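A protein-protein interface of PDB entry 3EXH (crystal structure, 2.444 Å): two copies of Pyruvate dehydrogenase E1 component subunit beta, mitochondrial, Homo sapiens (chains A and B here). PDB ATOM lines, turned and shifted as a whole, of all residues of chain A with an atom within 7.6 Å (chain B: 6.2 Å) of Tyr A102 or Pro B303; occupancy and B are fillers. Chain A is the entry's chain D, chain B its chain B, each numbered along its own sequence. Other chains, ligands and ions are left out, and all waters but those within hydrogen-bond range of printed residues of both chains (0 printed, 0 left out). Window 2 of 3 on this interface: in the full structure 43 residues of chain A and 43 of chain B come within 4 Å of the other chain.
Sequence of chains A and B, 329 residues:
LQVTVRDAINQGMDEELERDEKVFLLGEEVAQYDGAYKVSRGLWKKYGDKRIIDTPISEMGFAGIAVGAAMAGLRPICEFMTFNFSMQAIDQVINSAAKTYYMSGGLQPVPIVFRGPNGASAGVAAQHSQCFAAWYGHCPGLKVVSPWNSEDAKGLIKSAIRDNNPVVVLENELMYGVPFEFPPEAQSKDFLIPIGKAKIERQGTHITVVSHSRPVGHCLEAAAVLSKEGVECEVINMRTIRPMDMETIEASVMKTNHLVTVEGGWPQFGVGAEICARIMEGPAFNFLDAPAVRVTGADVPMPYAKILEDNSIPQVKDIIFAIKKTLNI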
ATOM      1  N   ALA A  97     -19.334 -16.782 -17.682  1.00  0.00           N
ATOM      2  CA  ALA A  97     -19.202 -17.707 -18.809  1.00  0.00           C
ATOM      3  C   ALA A  97     -19.107 -16.945 -20.110  1.00  0.00           C
ATOM      4  O   ALA A  97     -18.111 -17.079 -20.818  1.00  0.00           O
ATOM      5  CB  ALA A  97     -20.346 -18.729 -18.865  1.00  0.00           C
ATOM      6  N   ALA A  98     -20.148 -16.182 -20.461  1.00  0.00           N
ATOM      7  CA  ALA A  98     -20.199 -15.568 -21.803  1.00  0.00           C
ATOM      8  C   ALA A  98     -18.919 -14.749 -22.151  1.00  0.00           C
ATOM      9  O   ALA A  98     -18.368 -14.847 -23.240  1.00  0.00           O
ATOM     10  CB  ALA A  98     -21.433 -14.685 -21.920  1.00  0.00           C
ATOM     11  N   LYS A  99     -18.445 -13.938 -21.221  1.00  0.00           N
ATOM     12  CA  LYS A  99     -17.454 -12.910 -21.571  1.00  0.00           C
ATOM     13  C   LYS A  99     -15.997 -13.368 -21.459  1.00  0.00           C
ATOM     14  O   LYS A  99     -15.093 -12.694 -21.948  1.00  0.00           O
ATOM     15  CB  LYS A  99     -17.679 -11.640 -20.725  1.00  0.00           C
ATOM     16  CG  LYS A  99     -19.071 -11.034 -20.891  1.00  0.00           C
ATOM     17  CD  LYS A  99     -19.182  -9.703 -20.208  1.00  0.00           C
ATOM     18  CE  LYS A  99     -20.633  -9.313 -20.151  1.00  0.00           C
ATOM     19  NZ  LYS A  99     -20.967  -8.195 -19.179  1.00  0.00           N
ATOM     20  N   THR A 100     -15.788 -14.513 -20.822  1.00  0.00           N
ATOM     21  CA  THR A 100     -14.472 -14.925 -20.377  1.00  0.00           C
ATOM     22  C   THR A 100     -13.533 -15.289 -21.465  1.00  0.00           C
ATOM     23  O   THR A 100     -12.347 -14.952 -21.396  1.00  0.00           O
ATOM     24  CB  THR A 100     -14.573 -16.108 -19.427  1.00  0.00           C
ATOM     25  OG1 THR A 100     -15.220 -15.638 -18.231  1.00  0.00           O
ATOM     26  CG2 THR A 100     -13.188 -16.623 -19.107  1.00  0.00           C
ATOM     27  N   TYR A 101     -14.006 -15.985 -22.491  1.00  0.00           N
ATOM     28  CA  TYR A 101     -13.048 -16.243 -23.570  1.00  0.00           C
ATOM     29  C   TYR A 101     -12.498 -14.914 -24.127  1.00  0.00           C
ATOM     30  O   TYR A 101     -11.319 -14.780 -24.357  1.00  0.00           O
ATOM     31  CB  TYR A 101     -13.644 -17.092 -24.689  1.00  0.00           C
ATOM     32  CG  TYR A 101     -12.634 -17.680 -25.660  1.00  0.00           C
ATOM     33  CD1 TYR A 101     -11.729 -18.659 -25.254  1.00  0.00           C
ATOM     34  CD2 TYR A 101     -12.636 -17.291 -27.002  1.00  0.00           C
ATOM     35  CE1 TYR A 101     -10.833 -19.229 -26.174  1.00  0.00           C
ATOM     36  CE2 TYR A 101     -11.755 -17.809 -27.894  1.00  0.00           C
ATOM     37  CZ  TYR A 101     -10.861 -18.792 -27.484  1.00  0.00           C
ATOM     38  OH  TYR A 101     -10.011 -19.340 -28.416  1.00  0.00           O
ATOM     39  N   TYR A 102     -13.371 -13.949 -24.350  1.00  0.00           N
ATOM     40  CA  TYR A 102     -12.931 -12.720 -24.896  1.00  0.00           C
ATOM     41  C   TYR A 102     -11.986 -12.057 -23.918  1.00  0.00           C
ATOM     42  O   TYR A 102     -10.931 -11.601 -24.328  1.00  0.00           O
ATOM     43  CB  TYR A 102     -14.118 -11.806 -25.149  1.00  0.00           C
ATOM     44  CG  TYR A 102     -13.790 -10.550 -25.896  1.00  0.00           C
ATOM     45  CD1 TYR A 102     -13.756 -10.531 -27.308  1.00  0.00           C
ATOM     46  CD2 TYR A 102     -13.619  -9.350 -25.220  1.00  0.00           C
ATOM     47  CE1 TYR A 102     -13.506  -9.338 -28.024  1.00  0.00           C
ATOM     48  CE2 TYR A 102     -13.343  -8.147 -25.916  1.00  0.00           C
ATOM     49  CZ  TYR A 102     -13.312  -8.156 -27.299  1.00  0.00           C
ATOM     50  OH  TYR A 102     -13.034  -6.987 -27.962  1.00  0.00           O
ATOM     51  N   MET A 103     -12.361 -11.990 -22.642  1.00  0.00           N
ATOM     52  CA  MET A 103     -11.557 -11.202 -21.691  1.00  0.00           C
ATOM     53  C   MET A 103     -10.179 -11.819 -21.506  1.00  0.00           C
ATOM     54  O   MET A 103      -9.227 -11.120 -21.280  1.00  0.00           O
ATOM     55  CB  MET A 103     -12.215 -11.046 -20.341  1.00  0.00           C
ATOM     56  CG  MET A 103     -13.432 -10.153 -20.329  1.00  0.00           C
ATOM     57  SD  MET A 103     -13.988  -9.890 -18.605  1.00  0.00           S
ATOM     58  CE  MET A 103     -14.268 -11.631 -18.198  1.00  0.00           C
ATOM     59  N   SER A 104     -10.069 -13.123 -21.646  1.00  0.00           N
ATOM     60  CA  SER A 104      -8.806 -13.754 -21.405  1.00  0.00           C
ATOM     61  C   SER A 104      -7.944 -13.729 -22.653  1.00  0.00           C
ATOM     62  O   SER A 104      -6.847 -14.272 -22.641  1.00  0.00           O
ATOM     63  CB  SER A 104      -9.038 -15.191 -20.982  1.00  0.00           C
ATOM     64  OG  SER A 104      -9.529 -15.975 -22.073  1.00  0.00           O
ATOM     65  N   GLY A 105      -8.425 -13.156 -23.761  1.00  0.00           N
ATOM     66  CA  GLY A 105      -7.576 -13.059 -24.972  1.00  0.00           C
ATOM     67  C   GLY A 105      -7.587 -14.370 -25.702  1.00  0.00           C
ATOM     68  O   GLY A 105      -6.818 -14.615 -26.636  1.00  0.00           O
ATOM     69  N   GLY A 106      -8.494 -15.243 -25.289  1.00  0.00           N
ATOM     70  CA  GLY A 106      -8.632 -16.521 -25.964  1.00  0.00           C
ATOM     71  C   GLY A 106      -7.912 -17.591 -25.178  1.00  0.00           C
ATOM     72  O   GLY A 106      -7.613 -18.640 -25.709  1.00  0.00           O
ATOM     73  N   LEU A 107      -7.641 -17.365 -23.895  1.00  0.00           N
ATOM     74  CA  LEU A 107      -6.941 -18.417 -23.171  1.00  0.00           C
ATOM     75  C   LEU A 107      -7.912 -19.329 -22.461  1.00  0.00           C
ATOM     76  O   LEU A 107      -7.633 -20.493 -22.245  1.00  0.00           O
ATOM     77  CB  LEU A 107      -5.913 -17.846 -22.189  1.00  0.00           C
ATOM     78  CG  LEU A 107      -5.030 -18.763 -21.275  1.00  0.00           C
ATOM     79  CD1 LEU A 107      -4.405 -20.109 -21.897  1.00  0.00           C
ATOM     80  CD2 LEU A 107      -3.854 -17.893 -20.694  1.00  0.00           C
ATOM     81  N   GLN A 108      -9.073 -18.827 -22.109  1.00  0.00           N
ATOM     82  CA  GLN A 108      -9.934 -19.634 -21.262  1.00  0.00           C
ATOM     83  C   GLN A 108     -11.302 -19.906 -21.909  1.00  0.00           C
ATOM     84  O   GLN A 108     -12.165 -19.054 -21.867  1.00  0.00           O
ATOM     85  CB  GLN A 108     -10.079 -18.926 -19.890  1.00  0.00           C
ATOM     86  CG  GLN A 108     -10.930 -19.622 -18.851  1.00  0.00           C
ATOM     87  CD  GLN A 108     -10.353 -20.976 -18.469  1.00  0.00           C
ATOM     88  OE1 GLN A 108      -9.388 -21.060 -17.689  1.00  0.00           O
ATOM     89  NE2 GLN A 108     -10.946 -22.057 -19.015  1.00  0.00           N
ATOM     90  N   PRO A 109     -11.480 -21.071 -22.539  1.00  0.00           N
ATOM     91  CA  PRO A 109     -12.786 -21.371 -23.110  1.00  0.00           C
ATOM     92  C   PRO A 109     -13.756 -21.836 -22.025  1.00  0.00           C
ATOM     93  O   PRO A 109     -13.332 -22.248 -20.952  1.00  0.00           O
ATOM     94  CB  PRO A 109     -12.516 -22.526 -24.095  1.00  0.00           C
ATOM     95  CG  PRO A 109     -11.078 -22.878 -23.980  1.00  0.00           C
ATOM     96  CD  PRO A 109     -10.487 -22.124 -22.814  1.00  0.00           C
ATOM     97  N   PRO A 140     -23.241 -10.895 -26.265  1.00  0.00           N
ATOM     98  CA  PRO A 140     -22.096 -11.428 -26.977  1.00  0.00           C
ATOM     99  C   PRO A 140     -21.388 -12.469 -26.100  1.00  0.00           C
ATOM    100  O   PRO A 140     -21.297 -12.294 -24.915  1.00  0.00           O
ATOM    101  CB  PRO A 140     -21.191 -10.196 -27.165  1.00  0.00           C
ATOM    102  CG  PRO A 140     -22.133  -9.025 -27.056  1.00  0.00           C
ATOM    103  CD  PRO A 140     -23.118  -9.451 -25.998  1.00  0.00           C
ATOM    104  N   GLY A 141     -20.870 -13.538 -26.702  1.00  0.00           N
ATOM    105  CA  GLY A 141     -20.140 -14.564 -25.950  1.00  0.00           C
ATOM    106  C   GLY A 141     -20.993 -15.796 -25.724  1.00  0.00           C
ATOM    107  O   GLY A 141     -20.489 -16.899 -25.434  1.00  0.00           O
ATOM    108  N   GLY B 123     -12.379   2.280 -19.689  1.00  0.00           N
ATOM    109  CA  GLY B 123     -11.382   1.314 -19.309  1.00  0.00           C
ATOM    110  C   GLY B 123     -11.773   0.377 -18.208  1.00  0.00           C
ATOM    111  O   GLY B 123     -10.908  -0.260 -17.641  1.00  0.00           O
ATOM    112  N   VAL B 124     -13.054   0.204 -17.933  1.00  0.00           N
ATOM    113  CA  VAL B 124     -13.413  -0.744 -16.900  1.00  0.00           C
ATOM    114  C   VAL B 124     -13.662  -2.160 -17.396  1.00  0.00           C
ATOM    115  O   VAL B 124     -13.902  -3.045 -16.611  1.00  0.00           O
ATOM    116  CB  VAL B 124     -14.622  -0.267 -16.147  1.00  0.00           C
ATOM    117  CG1 VAL B 124     -14.263   0.998 -15.394  1.00  0.00           C
ATOM    118  CG2 VAL B 124     -15.788   0.031 -17.114  1.00  0.00           C
ATOM    119  N   ALA B 125     -13.613  -2.366 -18.709  1.00  0.00           N
ATOM    120  CA  ALA B 125     -13.615  -3.691 -19.331  1.00  0.00           C
ATOM    121  C   ALA B 125     -14.967  -4.461 -19.251  1.00  0.00           C
ATOM    122  O   ALA B 125     -15.990  -3.873 -18.869  1.00  0.00           O
ATOM    123  CB  ALA B 125     -12.489  -4.493 -18.836  1.00  0.00           C
ATOM    124  N   ALA B 126     -14.985  -5.733 -19.628  1.00  0.00           N
ATOM    125  CA  ALA B 126     -16.257  -6.358 -20.017  1.00  0.00           C
ATOM    126  C   ALA B 126     -17.283  -6.560 -18.917  1.00  0.00           C
ATOM    127  O   ALA B 126     -18.471  -6.391 -19.161  1.00  0.00           O
ATOM    128  CB  ALA B 126     -16.027  -7.672 -20.760  1.00  0.00           C
ATOM    129  N   VAL B 300     -19.591  -6.819 -28.948  1.00  0.00           N
ATOM    130  CA  VAL B 300     -18.511  -7.549 -28.256  1.00  0.00           C
ATOM    131  C   VAL B 300     -18.591  -7.241 -26.785  1.00  0.00           C
ATOM    132  O   VAL B 300     -19.145  -6.196 -26.386  1.00  0.00           O
ATOM    133  CB  VAL B 300     -17.095  -7.141 -28.747  1.00  0.00           C
ATOM    134  CG1 VAL B 300     -16.933  -7.595 -30.112  1.00  0.00           C
ATOM    135  CG2 VAL B 300     -16.923  -5.592 -28.682  1.00  0.00           C
ATOM    136  N   PRO B 301     -18.076  -8.157 -25.957  1.00  0.00           N
ATOM    137  CA  PRO B 301     -17.880  -7.763 -24.536  1.00  0.00           C
ATOM    138  C   PRO B 301     -16.833  -6.590 -24.598  1.00  0.00           C
ATOM    139  O   PRO B 301     -15.967  -6.567 -25.487  1.00  0.00           O
ATOM    140  CB  PRO B 301     -17.275  -9.009 -23.911  1.00  0.00           C
ATOM    141  CG  PRO B 301     -17.449 -10.155 -24.978  1.00  0.00           C
ATOM    142  CD  PRO B 301     -17.486  -9.471 -26.296  1.00  0.00           C
ATOM    143  N   MET B 302     -16.975  -5.606 -23.724  1.00  0.00           N
ATOM    144  CA  MET B 302     -16.205  -4.370 -23.827  1.00  0.00           C
ATOM    145  C   MET B 302     -14.714  -4.664 -23.613  1.00  0.00           C
ATOM    146  O   MET B 302     -14.325  -5.200 -22.557  1.00  0.00           O
ATOM    147  CB  MET B 302     -16.706  -3.361 -22.777  1.00  0.00           C
ATOM    148  CG  MET B 302     -16.045  -1.990 -22.867  1.00  0.00           C
ATOM    149  SD  MET B 302     -16.409  -1.224 -24.485  1.00  0.00           S
ATOM    150  CE  MET B 302     -18.139  -0.810 -24.178  1.00  0.00           C
ATOM    151  N   PRO B 303     -13.874  -4.369 -24.632  1.00  0.00           N
ATOM    152  CA  PRO B 303     -12.439  -4.584 -24.451  1.00  0.00           C
ATOM    153  C   PRO B 303     -11.768  -3.493 -23.584  1.00  0.00           C
ATOM    154  O   PRO B 303     -12.253  -2.379 -23.462  1.00  0.00           O
ATOM    155  CB  PRO B 303     -11.909  -4.509 -25.876  1.00  0.00           C
ATOM    156  CG  PRO B 303     -12.892  -3.494 -26.570  1.00  0.00           C
ATOM    157  CD  PRO B 303     -14.215  -3.850 -25.984  1.00  0.00           C
ATOM    158  N   TYR B 304     -10.639  -3.818 -22.988  1.00  0.00           N
ATOM    159  CA  TYR B 304      -9.926  -2.828 -22.164  1.00  0.00           C
ATOM    160  C   TYR B 304      -9.099  -1.782 -22.948  1.00  0.00           C
ATOM    161  O   TYR B 304      -9.179  -0.634 -22.663  1.00  0.00           O
ATOM    162  CB  TYR B 304      -9.001  -3.553 -21.185  1.00  0.00           C
ATOM    163  CG  TYR B 304      -8.108  -2.637 -20.412  1.00  0.00           C
ATOM    164  CD1 TYR B 304      -8.640  -1.755 -19.468  1.00  0.00           C
ATOM    165  CD2 TYR B 304      -6.746  -2.646 -20.604  1.00  0.00           C
ATOM    166  CE1 TYR B 304      -7.816  -0.908 -18.704  1.00  0.00           C
ATOM    167  CE2 TYR B 304      -5.908  -1.814 -19.851  1.00  0.00           C
ATOM    168  CZ  TYR B 304      -6.446  -0.946 -18.904  1.00  0.00           C
ATOM    169  OH  TYR B 304      -5.618  -0.130 -18.162  1.00  0.00           O
ATOM    170  N   ALA B 305      -8.261  -2.187 -23.876  1.00  0.00           N
ATOM    171  CA  ALA B 305      -7.297  -1.246 -24.487  1.00  0.00           C
ATOM    172  C   ALA B 305      -7.971  -0.031 -25.123  1.00  0.00           C
ATOM    173  O   ALA B 305      -8.964  -0.147 -25.830  1.00  0.00           O
ATOM    174  CB  ALA B 305      -6.429  -1.957 -25.532  1.00  0.00           C
ATOM    175  N   LYS B 306      -7.420   1.138 -24.891  1.00  0.00           N
ATOM    176  CA  LYS B 306      -8.076   2.359 -25.320  1.00  0.00           C
ATOM    177  C   LYS B 306      -8.636   2.326 -26.794  1.00  0.00           C
ATOM    178  O   LYS B 306      -9.822   2.542 -27.044  1.00  0.00           O
ATOM    179  CB  LYS B 306      -7.083   3.499 -25.168  1.00  0.00           C
ATOM    180  CG  LYS B 306      -7.789   4.706 -24.595  1.00  0.00           C
ATOM    181  CD  LYS B 306      -8.048   5.700 -25.668  1.00  0.00           C
ATOM    182  CE  LYS B 306      -8.421   7.097 -25.090  1.00  0.00           C
ATOM    183  NZ  LYS B 306      -9.871   7.183 -24.828  1.00  0.00           N
ATOM    184  N   LEU B 308      -9.325  -0.067 -28.733  1.00  0.00           N
ATOM    185  CA  LEU B 308     -10.415  -1.020 -28.888  1.00  0.00           C
ATOM    186  C   LEU B 308     -11.748  -0.491 -28.291  1.00  0.00           C
ATOM    187  O   LEU B 308     -12.808  -0.569 -28.911  1.00  0.00           O
ATOM    188  CB  LEU B 308     -10.032  -2.355 -28.291  1.00  0.00           C
ATOM    189  CG  LEU B 308      -8.701  -2.924 -28.811  1.00  0.00           C
ATOM    190  CD1 LEU B 308      -8.476  -4.297 -28.229  1.00  0.00           C
ATOM    191  CD2 LEU B 308      -8.645  -2.983 -30.311  1.00  0.00           C
ATOM    192  N   GLU B 309     -11.677   0.103 -27.103  1.00  0.00           N
ATOM    193  CA  GLU B 309     -12.829   0.639 -26.464  1.00  0.00           C
ATOM    194  C   GLU B 309     -13.448   1.796 -27.246  1.00  0.00           C
ATOM    195  O   GLU B 309     -14.675   1.909 -27.331  1.00  0.00           O
ATOM    196  CB  GLU B 309     -12.445   1.108 -25.078  1.00  0.00           C
ATOM    197  CG  GLU B 309     -13.654   1.504 -24.287  1.00  0.00           C
ATOM    198  CD  GLU B 309     -13.302   2.066 -22.949  1.00  0.00           C
ATOM    199  OE1 GLU B 309     -12.327   2.808 -22.860  1.00  0.00           O
ATOM    200  OE2 GLU B 309     -14.019   1.769 -21.996  1.00  0.00           O
ATOM    201  N   SER B 312     -15.654   0.592 -29.730  1.00  0.00           N
ATOM    202  CA  SER B 312     -16.669  -0.271 -29.238  1.00  0.00           C
ATOM    203  C   SER B 312     -17.941   0.440 -28.794  1.00  0.00           C
ATOM    204  O   SER B 312     -18.939  -0.198 -28.480  1.00  0.00           O
ATOM    205  CB  SER B 312     -16.095  -1.093 -28.120  1.00  0.00           C
ATOM    206  OG  SER B 312     -15.238  -2.030 -28.673  1.00  0.00           O
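The backbone carbonyl oxygen of Ala B126 lies within hydrogen-bond range of the side-chain amino group of Lys A99 (3.1 Å).
N of Ala B126 is in hydrogen-bond range of O of Met B302.
Among the printed residues, merely in contact across the chains: Tyr A102 with Pro B301, Tyr A102 with Pro B303, Met A103 with Ala B126, Pro A140 with Val B300 and Pro A140 with Pro B301.
Tyr A102 touches just these residues of chain B: Pro B301 and Pro B303. Of chain A, only Tyr A102 comes within 4 Å of Pro B303. Of the printed residues of chain A, Pro B301 touches Tyr A102 and Pro A140. Of the printed residues of chain B, Pro A140 touches Val B300 and Pro B301. Of the printed residues of chain A, Val B300 touches Pro A140 (3.9 Å). Thr A100 touches none of the printed residues of chain B. Glu B309 touches none of the printed residues of chain A. The nearest residue of chain A that does not touch Pro B303 is Met A103 (7.0 Å).
Printed residues of chain B that touch a printed residue of chain A: Ala B126, Val B300, Pro B301 and Pro B303. Hydrophobic or aromatic side chains of chain A within 4 Å of the printed part of chain B: Tyr A102, Met A103 and Pro A140. Among the printed residues, no Asp or Glu carboxylate lies within 4 Å of a Lys or Arg side-chain nitrogen of the other chain.
No position is printed for both chains.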
